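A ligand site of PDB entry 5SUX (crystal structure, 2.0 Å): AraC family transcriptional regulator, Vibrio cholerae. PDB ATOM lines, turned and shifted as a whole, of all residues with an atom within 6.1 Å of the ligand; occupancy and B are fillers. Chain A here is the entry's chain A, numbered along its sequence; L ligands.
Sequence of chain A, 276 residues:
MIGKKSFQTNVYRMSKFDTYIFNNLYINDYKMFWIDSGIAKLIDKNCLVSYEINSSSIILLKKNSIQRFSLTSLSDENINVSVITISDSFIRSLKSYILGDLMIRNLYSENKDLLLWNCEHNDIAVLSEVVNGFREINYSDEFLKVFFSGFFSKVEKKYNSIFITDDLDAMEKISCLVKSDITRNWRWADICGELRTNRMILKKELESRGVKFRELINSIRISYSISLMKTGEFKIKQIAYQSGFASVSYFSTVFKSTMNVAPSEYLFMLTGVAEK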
ATOM      1  N   GLN A   8     -24.894  24.333  15.147  1.00  0.00           N
ATOM      2  CA  GLN A   8     -23.610  23.899  14.614  1.00  0.00           C
ATOM      3  C   GLN A   8     -22.774  23.402  15.784  1.00  0.00           C
ATOM      4  O   GLN A   8     -22.641  24.107  16.795  1.00  0.00           O
ATOM      5  CB  GLN A   8     -22.895  25.024  13.871  1.00  0.00           C
ATOM      6  CG  GLN A   8     -21.703  24.581  13.038  1.00  0.00           C
ATOM      7  CD  GLN A   8     -20.463  24.332  13.869  1.00  0.00           C
ATOM      8  OE1 GLN A   8     -20.253  24.970  14.899  1.00  0.00           O
ATOM      9  NE2 GLN A   8     -19.638  23.385  13.429  1.00  0.00           N
ATOM     10  N   ASN A  10     -19.322  20.982  17.403  1.00  0.00           N
ATOM     11  CA  ASN A  10     -17.975  20.453  17.257  1.00  0.00           C
ATOM     12  C   ASN A  10     -17.543  19.840  18.583  1.00  0.00           C
ATOM     13  O   ASN A  10     -18.006  20.246  19.653  1.00  0.00           O
ATOM     14  CB  ASN A  10     -16.979  21.545  16.833  1.00  0.00           C
ATOM     15  CG  ASN A  10     -17.166  21.979  15.399  1.00  0.00           C
ATOM     16  OD1 ASN A  10     -17.665  23.080  15.134  1.00  0.00           O
ATOM     17  ND2 ASN A  10     -16.764  21.131  14.460  1.00  0.00           N
ATOM     18  N   TYR A  12     -13.902  18.747  20.596  1.00  0.00           N
ATOM     19  CA  TYR A  12     -12.457  18.920  20.602  1.00  0.00           C
ATOM     20  C   TYR A  12     -11.843  18.081  21.720  1.00  0.00           C
ATOM     21  O   TYR A  12     -12.463  17.892  22.770  1.00  0.00           O
ATOM     22  CB  TYR A  12     -12.084  20.389  20.811  1.00  0.00           C
ATOM     23  CG  TYR A  12     -12.727  21.327  19.821  1.00  0.00           C
ATOM     24  CD1 TYR A  12     -12.159  21.556  18.578  1.00  0.00           C
ATOM     25  CD2 TYR A  12     -13.900  21.995  20.130  1.00  0.00           C
ATOM     26  CE1 TYR A  12     -12.740  22.415  17.668  1.00  0.00           C
ATOM     27  CE2 TYR A  12     -14.493  22.854  19.227  1.00  0.00           C
ATOM     28  CZ  TYR A  12     -13.910  23.070  17.994  1.00  0.00           C
ATOM     29  OH  TYR A  12     -14.495  23.924  17.092  1.00  0.00           O
ATOM     30  N   TYR A  20      -6.353  25.382  25.939  1.00  0.00           N
ATOM     31  CA  TYR A  20      -6.837  26.257  24.884  1.00  0.00           C
ATOM     32  C   TYR A  20      -6.892  27.681  25.412  1.00  0.00           C
ATOM     33  O   TYR A  20      -7.354  27.920  26.536  1.00  0.00           O
ATOM     34  CB  TYR A  20      -8.230  25.830  24.416  1.00  0.00           C
ATOM     35  CG  TYR A  20      -8.275  24.520  23.653  1.00  0.00           C
ATOM     36  CD1 TYR A  20      -8.886  23.403  24.187  1.00  0.00           C
ATOM     37  CD2 TYR A  20      -7.697  24.411  22.395  1.00  0.00           C
ATOM     38  CE1 TYR A  20      -8.934  22.207  23.499  1.00  0.00           C
ATOM     39  CE2 TYR A  20      -7.728  23.220  21.692  1.00  0.00           C
ATOM     40  CZ  TYR A  20      -8.359  22.117  22.251  1.00  0.00           C
ATOM     41  OH  TYR A  20      -8.391  20.929  21.562  1.00  0.00           O
ATOM     42  N   PHE A  22      -7.825  31.741  24.302  1.00  0.00           N
ATOM     43  CA  PHE A  22      -8.522  32.603  23.357  1.00  0.00           C
ATOM     44  C   PHE A  22      -8.348  34.048  23.773  1.00  0.00           C
ATOM     45  O   PHE A  22      -8.522  34.393  24.943  1.00  0.00           O
ATOM     46  CB  PHE A  22      -9.994  32.223  23.259  1.00  0.00           C
ATOM     47  CG  PHE A  22     -10.214  30.777  22.921  1.00  0.00           C
ATOM     48  CD1 PHE A  22      -9.979  30.312  21.637  1.00  0.00           C
ATOM     49  CD2 PHE A  22     -10.614  29.872  23.894  1.00  0.00           C
ATOM     50  CE1 PHE A  22     -10.172  28.979  21.324  1.00  0.00           C
ATOM     51  CE2 PHE A  22     -10.797  28.535  23.583  1.00  0.00           C
ATOM     52  CZ  PHE A  22     -10.574  28.090  22.294  1.00  0.00           C
ATOM     53  N   LEU A  25     -11.549  36.834  21.062  1.00  0.00           N
ATOM     54  CA  LEU A  25     -12.417  35.935  20.306  1.00  0.00           C
ATOM     55  C   LEU A  25     -13.797  36.548  20.204  1.00  0.00           C
ATOM     56  O   LEU A  25     -14.527  36.630  21.201  1.00  0.00           O
ATOM     57  CB  LEU A  25     -12.478  34.553  20.948  1.00  0.00           C
ATOM     58  CG  LEU A  25     -13.362  33.551  20.200  1.00  0.00           C
ATOM     59  CD1 LEU A  25     -12.778  33.253  18.827  1.00  0.00           C
ATOM     60  CD2 LEU A  25     -13.553  32.279  21.007  1.00  0.00           C
ATOM     61  N   ILE A  27     -17.608  36.558  19.443  1.00  0.00           N
ATOM     62  CA  ILE A  27     -18.665  35.547  19.497  1.00  0.00           C
ATOM     63  C   ILE A  27     -19.739  35.977  18.506  1.00  0.00           C
ATOM     64  O   ILE A  27     -20.533  36.890  18.781  1.00  0.00           O
ATOM     65  CB  ILE A  27     -19.211  35.376  20.916  1.00  0.00           C
ATOM     66  CG1 ILE A  27     -18.063  35.074  21.887  1.00  0.00           C
ATOM     67  CG2 ILE A  27     -20.239  34.263  20.974  1.00  0.00           C
ATOM     68  CD1 ILE A  27     -17.299  33.814  21.540  1.00  0.00           C
ATOM     69  N   ASN A  28     -19.784  35.317  17.351  1.00  0.00           N
ATOM     70  CA  ASN A  28     -20.685  35.706  16.276  1.00  0.00           C
ATOM     71  C   ASN A  28     -22.096  35.166  16.444  1.00  0.00           C
ATOM     72  O   ASN A  28     -23.028  35.682  15.817  1.00  0.00           O
ATOM     73  CB  ASN A  28     -20.134  35.251  14.923  1.00  0.00           C
ATOM     74  CG  ASN A  28     -20.076  33.750  14.791  1.00  0.00           C
ATOM     75  OD1 ASN A  28     -19.740  33.049  15.748  1.00  0.00           O
ATOM     76  ND2 ASN A  28     -20.405  33.237  13.611  1.00  0.00           N
ATOM     77  N   LYS A  31     -23.150  30.680  21.960  1.00  0.00           N
ATOM     78  CA  LYS A  31     -22.428  29.436  22.080  1.00  0.00           C
ATOM     79  C   LYS A  31     -22.543  28.901  23.502  1.00  0.00           C
ATOM     80  O   LYS A  31     -22.754  29.662  24.448  1.00  0.00           O
ATOM     81  CB  LYS A  31     -20.947  29.591  21.714  1.00  0.00           C
ATOM     82  CG  LYS A  31     -20.682  29.966  20.278  1.00  0.00           C
ATOM     83  CD  LYS A  31     -19.184  30.122  20.030  1.00  0.00           C
ATOM     84  CE  LYS A  31     -18.921  31.014  18.821  1.00  0.00           C
ATOM     85  NZ  LYS A  31     -19.287  30.348  17.551  1.00  0.00           N
ATOM     86  N   PHE A  33     -20.585  25.497  25.847  1.00  0.00           N
ATOM     87  CA  PHE A  33     -19.669  24.358  25.827  1.00  0.00           C
ATOM     88  C   PHE A  33     -19.581  23.719  27.202  1.00  0.00           C
ATOM     89  O   PHE A  33     -19.932  24.325  28.223  1.00  0.00           O
ATOM     90  CB  PHE A  33     -18.269  24.765  25.312  1.00  0.00           C
ATOM     91  CG  PHE A  33     -17.530  25.722  26.216  1.00  0.00           C
ATOM     92  CD1 PHE A  33     -17.585  27.090  25.994  1.00  0.00           C
ATOM     93  CD2 PHE A  33     -16.733  25.239  27.244  1.00  0.00           C
ATOM     94  CE1 PHE A  33     -16.882  27.963  26.801  1.00  0.00           C
ATOM     95  CE2 PHE A  33     -16.031  26.112  28.050  1.00  0.00           C
ATOM     96  CZ  PHE A  33     -16.098  27.480  27.835  1.00  0.00           C
ATOM     97  N   LEU A  61     -21.672  31.562  26.317  1.00  0.00           N
ATOM     98  CA  LEU A  61     -20.951  32.692  25.762  1.00  0.00           C
ATOM     99  C   LEU A  61     -21.928  33.589  25.000  1.00  0.00           C
ATOM    100  O   LEU A  61     -22.606  33.132  24.083  1.00  0.00           O
ATOM    101  CB  LEU A  61     -19.821  32.230  24.843  1.00  0.00           C
ATOM    102  CG  LEU A  61     -18.764  31.323  25.487  1.00  0.00           C
ATOM    103  CD1 LEU A  61     -17.710  30.926  24.462  1.00  0.00           C
ATOM    104  CD2 LEU A  61     -18.126  32.000  26.693  1.00  0.00           C
ATOM    105  N   PHE A  69     -10.153  34.100  27.522  1.00  0.00           N
ATOM    106  CA  PHE A  69     -10.141  33.073  28.564  1.00  0.00           C
ATOM    107  C   PHE A  69      -9.299  31.897  28.113  1.00  0.00           C
ATOM    108  O   PHE A  69      -9.006  31.728  26.922  1.00  0.00           O
ATOM    109  CB  PHE A  69     -11.571  32.623  28.921  1.00  0.00           C
ATOM    110  CG  PHE A  69     -12.252  31.825  27.836  1.00  0.00           C
ATOM    111  CD1 PHE A  69     -12.960  32.454  26.829  1.00  0.00           C
ATOM    112  CD2 PHE A  69     -12.193  30.438  27.830  1.00  0.00           C
ATOM    113  CE1 PHE A  69     -13.587  31.727  25.832  1.00  0.00           C
ATOM    114  CE2 PHE A  69     -12.826  29.702  26.849  1.00  0.00           C
ATOM    115  CZ  PHE A  69     -13.517  30.347  25.847  1.00  0.00           C
ATOM    116  N   LEU A  71      -8.742  27.479  28.964  1.00  0.00           N
ATOM    117  CA  LEU A  71      -9.334  26.267  29.515  1.00  0.00           C
ATOM    118  C   LEU A  71      -8.252  25.196  29.565  1.00  0.00           C
ATOM    119  O   LEU A  71      -7.653  24.876  28.540  1.00  0.00           O
ATOM    120  CB  LEU A  71     -10.520  25.797  28.658  1.00  0.00           C
ATOM    121  CG  LEU A  71     -11.325  24.596  29.175  1.00  0.00           C
ATOM    122  CD1 LEU A  71     -11.991  24.919  30.503  1.00  0.00           C
ATOM    123  CD2 LEU A  71     -12.360  24.174  28.139  1.00  0.00           C
ATOM    124  N   VAL A  81     -14.274  18.290  24.722  1.00  0.00           N
ATOM    125  CA  VAL A  81     -15.002  19.541  24.884  1.00  0.00           C
ATOM    126  C   VAL A  81     -15.993  19.669  23.735  1.00  0.00           C
ATOM    127  O   VAL A  81     -15.596  19.654  22.563  1.00  0.00           O
ATOM    128  CB  VAL A  81     -14.056  20.747  24.917  1.00  0.00           C
ATOM    129  CG1 VAL A  81     -14.812  22.009  25.293  1.00  0.00           C
ATOM    130  CG2 VAL A  81     -12.907  20.494  25.891  1.00  0.00           C
ATOM    131  N   VAL A  83     -18.817  21.918  21.784  1.00  0.00           N
ATOM    132  CA  VAL A  83     -19.194  23.310  21.550  1.00  0.00           C
ATOM    133  C   VAL A  83     -20.401  23.336  20.620  1.00  0.00           C
ATOM    134  O   VAL A  83     -20.358  22.745  19.539  1.00  0.00           O
ATOM    135  CB  VAL A  83     -18.045  24.128  20.963  1.00  0.00           C
ATOM    136  CG1 VAL A  83     -18.446  25.589  20.807  1.00  0.00           C
ATOM    137  CG2 VAL A  83     -16.794  24.011  21.837  1.00  0.00           C
ATOM    138  N   THR A  85     -22.976  25.944  18.595  1.00  0.00           N
ATOM    139  CA  THR A  85     -23.261  27.285  18.115  1.00  0.00           C
ATOM    140  C   THR A  85     -24.706  27.337  17.648  1.00  0.00           C
ATOM    141  O   THR A  85     -25.110  26.538  16.801  1.00  0.00           O
ATOM    142  CB  THR A  85     -22.315  27.685  16.978  1.00  0.00           C
ATOM    143  OG1 THR A  85     -20.957  27.533  17.414  1.00  0.00           O
ATOM    144  CG2 THR A  85     -22.545  29.143  16.575  1.00  0.00           C
ATOM    145  N   SER A 223     -13.692  35.212  13.245  1.00  0.00           N
ATOM    146  CA  SER A 223     -14.849  34.355  13.477  1.00  0.00           C
ATOM    147  C   SER A 223     -15.594  34.061  12.184  1.00  0.00           C
ATOM    148  O   SER A 223     -16.223  32.998  12.058  1.00  0.00           O
ATOM    149  CB  SER A 223     -15.794  35.002  14.492  1.00  0.00           C
ATOM    150  OG  SER A 223     -15.276  34.875  15.809  1.00  0.00           O
ATOM    151  N   ILE A 226     -13.688  31.250  10.680  1.00  0.00           N
ATOM    152  CA  ILE A 226     -13.962  30.008  11.396  1.00  0.00           C
ATOM    153  C   ILE A 226     -15.259  29.374  10.901  1.00  0.00           C
ATOM    154  O   ILE A 226     -15.347  28.159  10.710  1.00  0.00           O
ATOM    155  CB  ILE A 226     -13.983  30.269  12.911  1.00  0.00           C
ATOM    156  CG1 ILE A 226     -12.573  30.534  13.419  1.00  0.00           C
ATOM    157  CG2 ILE A 226     -14.629  29.102  13.660  1.00  0.00           C
ATOM    158  CD1 ILE A 226     -12.506  31.000  14.853  1.00  0.00           C
ATOM    159  N   LYS A 230     -15.748  25.699   9.083  1.00  0.00           N
ATOM    160  CA  LYS A 230     -16.707  24.737   9.595  1.00  0.00           C
ATOM    161  C   LYS A 230     -17.551  24.129   8.487  1.00  0.00           C
ATOM    162  O   LYS A 230     -18.052  23.003   8.636  1.00  0.00           O
ATOM    163  CB  LYS A 230     -17.603  25.385  10.654  1.00  0.00           C
ATOM    164  CG  LYS A 230     -16.941  25.573  12.013  1.00  0.00           C
ATOM    165  CD  LYS A 230     -17.820  26.380  12.949  1.00  0.00           C
ATOM    166  CE  LYS A 230     -17.303  26.335  14.384  1.00  0.00           C
ATOM    167  NZ  LYS A 230     -18.142  27.172  15.293  1.00  0.00           N
ATOM    168  N   MET A 259      -6.552  32.461  18.407  1.00  0.00           N
ATOM    169  CA  MET A 259      -6.901  31.084  18.687  1.00  0.00           C
ATOM    170  C   MET A 259      -5.759  30.270  19.283  1.00  0.00           C
ATOM    171  O   MET A 259      -6.003  29.154  19.753  1.00  0.00           O
ATOM    172  CB  MET A 259      -7.379  30.391  17.404  1.00  0.00           C
ATOM    173  CG  MET A 259      -8.583  31.057  16.760  1.00  0.00           C
ATOM    174  SD  MET A 259     -10.098  30.781  17.691  1.00  0.00           S
ATOM    175  CE  MET A 259     -10.382  29.040  17.368  1.00  0.00           C
ATOM    176  N   TYR A 266      -6.215  24.401  13.119  1.00  0.00           N
ATOM    177  CA  TYR A 266      -7.615  24.427  13.510  1.00  0.00           C
ATOM    178  C   TYR A 266      -8.487  23.713  12.478  1.00  0.00           C
ATOM    179  O   TYR A 266      -9.443  23.014  12.834  1.00  0.00           O
ATOM    180  CB  TYR A 266      -8.108  25.858  13.713  1.00  0.00           C
ATOM    181  CG  TYR A 266      -9.552  25.902  14.157  1.00  0.00           C
ATOM    182  CD1 TYR A 266     -10.553  26.339  13.299  1.00  0.00           C
ATOM    183  CD2 TYR A 266      -9.913  25.485  15.432  1.00  0.00           C
ATOM    184  CE1 TYR A 266     -11.875  26.368  13.701  1.00  0.00           C
ATOM    185  CE2 TYR A 266     -11.232  25.522  15.839  1.00  0.00           C
ATOM    186  CZ  TYR A 266     -12.203  25.951  14.977  1.00  0.00           C
ATOM    187  OH  TYR A 266     -13.516  25.979  15.394  1.00  0.00           O
ATOM    188  N   MET A 269      -8.389  20.242  13.276  1.00  0.00           N
ATOM    189  CA  MET A 269      -9.158  19.979  14.490  1.00  0.00           C
ATOM    190  C   MET A 269     -10.643  19.812  14.189  1.00  0.00           C
ATOM    191  O   MET A 269     -11.343  19.082  14.890  1.00  0.00           O
ATOM    192  CB  MET A 269      -8.961  21.105  15.506  1.00  0.00           C
ATOM    193  CG  MET A 269      -7.586  21.128  16.155  1.00  0.00           C
ATOM    194  SD  MET A 269      -7.308  22.623  17.132  1.00  0.00           S
ATOM    195  CE  MET A 269      -8.878  22.769  17.983  1.00  0.00           C
HETATM  196  C1  LIG L   1     -13.904  27.622  18.393  1.00  0.00           C
HETATM  197  C2  LIG L   1     -14.565  28.693  17.568  1.00  0.00           C
HETATM  198  C3  LIG L   1     -16.063  28.472  17.476  1.00  0.00           C
HETATM  199  C4  LIG L   1     -12.878  25.024  23.970  1.00  0.00           C
HETATM  200  C5  LIG L   1     -15.302  28.240  22.470  1.00  0.00           C
HETATM  201  C6  LIG L   1     -14.402  27.087  22.874  1.00  0.00           C
HETATM  202  C7  LIG L   1     -13.476  26.378  22.012  1.00  0.00           C
HETATM  203  C8  LIG L   1     -12.737  25.367  22.586  1.00  0.00           C
HETATM  204  C9  LIG L   1     -11.793  24.593  21.842  1.00  0.00           C
HETATM  205  C10 LIG L   1     -11.588  24.848  20.497  1.00  0.00           C
HETATM  206  C11 LIG L   1     -12.308  25.868  19.899  1.00  0.00           C
HETATM  207  C12 LIG L   1     -13.238  26.633  20.596  1.00  0.00           C
HETATM  208  C13 LIG L   1     -13.919  27.701  19.748  1.00  0.00           C
HETATM  209  O1  LIG L   1     -16.817  29.408  17.122  1.00  0.00           O
HETATM  210  O2  LIG L   1     -16.561  27.346  17.748  1.00  0.00           O
HETATM  211  C14 LIG L   1     -13.762  25.708  24.774  1.00  0.00           C
HETATM  212  C15 LIG L   1     -14.517  26.738  24.216  1.00  0.00           C
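OG1 of Thr 85 sits at hydrogen-bond distance from NZ of Lys 31 (3.3 Å). The backbone NH of Leu 71 is in hydrogen-bond range of the backbone carbonyl oxygen of Tyr 20 (2.8 Å). The side-chain amide oxygen (OE1) of Gln 8 is in hydrogen-bond range of the side-chain amino group (NZ) of Lys 230. O of Tyr 12 sits at hydrogen-bond distance from N of Val 81. The backbone NH (N) of Val 83 lies within hydrogen-bond range of the backbone carbonyl oxygen (O) of Asn 10, 2.8 Å away. The backbone carbonyl oxygen (O) of Phe 69 is in hydrogen-bond range of the backbone NH (N) of Phe 22 (2.9 Å). The side-chain hydroxyl (OH) of Tyr 266 is in hydrogen-bond range of the side-chain hydroxyl (OH) of Tyr 12 (2.8 Å). The side-chain amino group (NZ) of Lys 31 sits at hydrogen-bond distance from the side-chain amide oxygen (OD1) of Asn 28 (3.3 Å).
NZ of Lys 230 is in salt-bridge range of O2 of the ligand (2.9 Å). NZ of Lys 31 is in salt-bridge range of O1 of the ligand (2.7 Å).
Residues that only touch the ligand: Tyr 12 (3.7 Å), Tyr 20 (3.9 Å), Phe 22 (3.4 Å), Phe 33 (3.6 Å), Leu 71 (3.95 Å), Val 81 (3.8 Å), Val 83 (3.9997 Å), Ile 226 (3.9 Å), Met 259 (3.9 Å) and Tyr 266 (3.4 Å). Hydrophobic or aromatic side chains within 4 Å of the ligand: Tyr 12, Tyr 20, Phe 22, Phe 33, Leu 71, Val 81, Val 83, Ile 226 and Met 259. Of the 22 residues printed, 12 come within 4 Å of the ligand.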
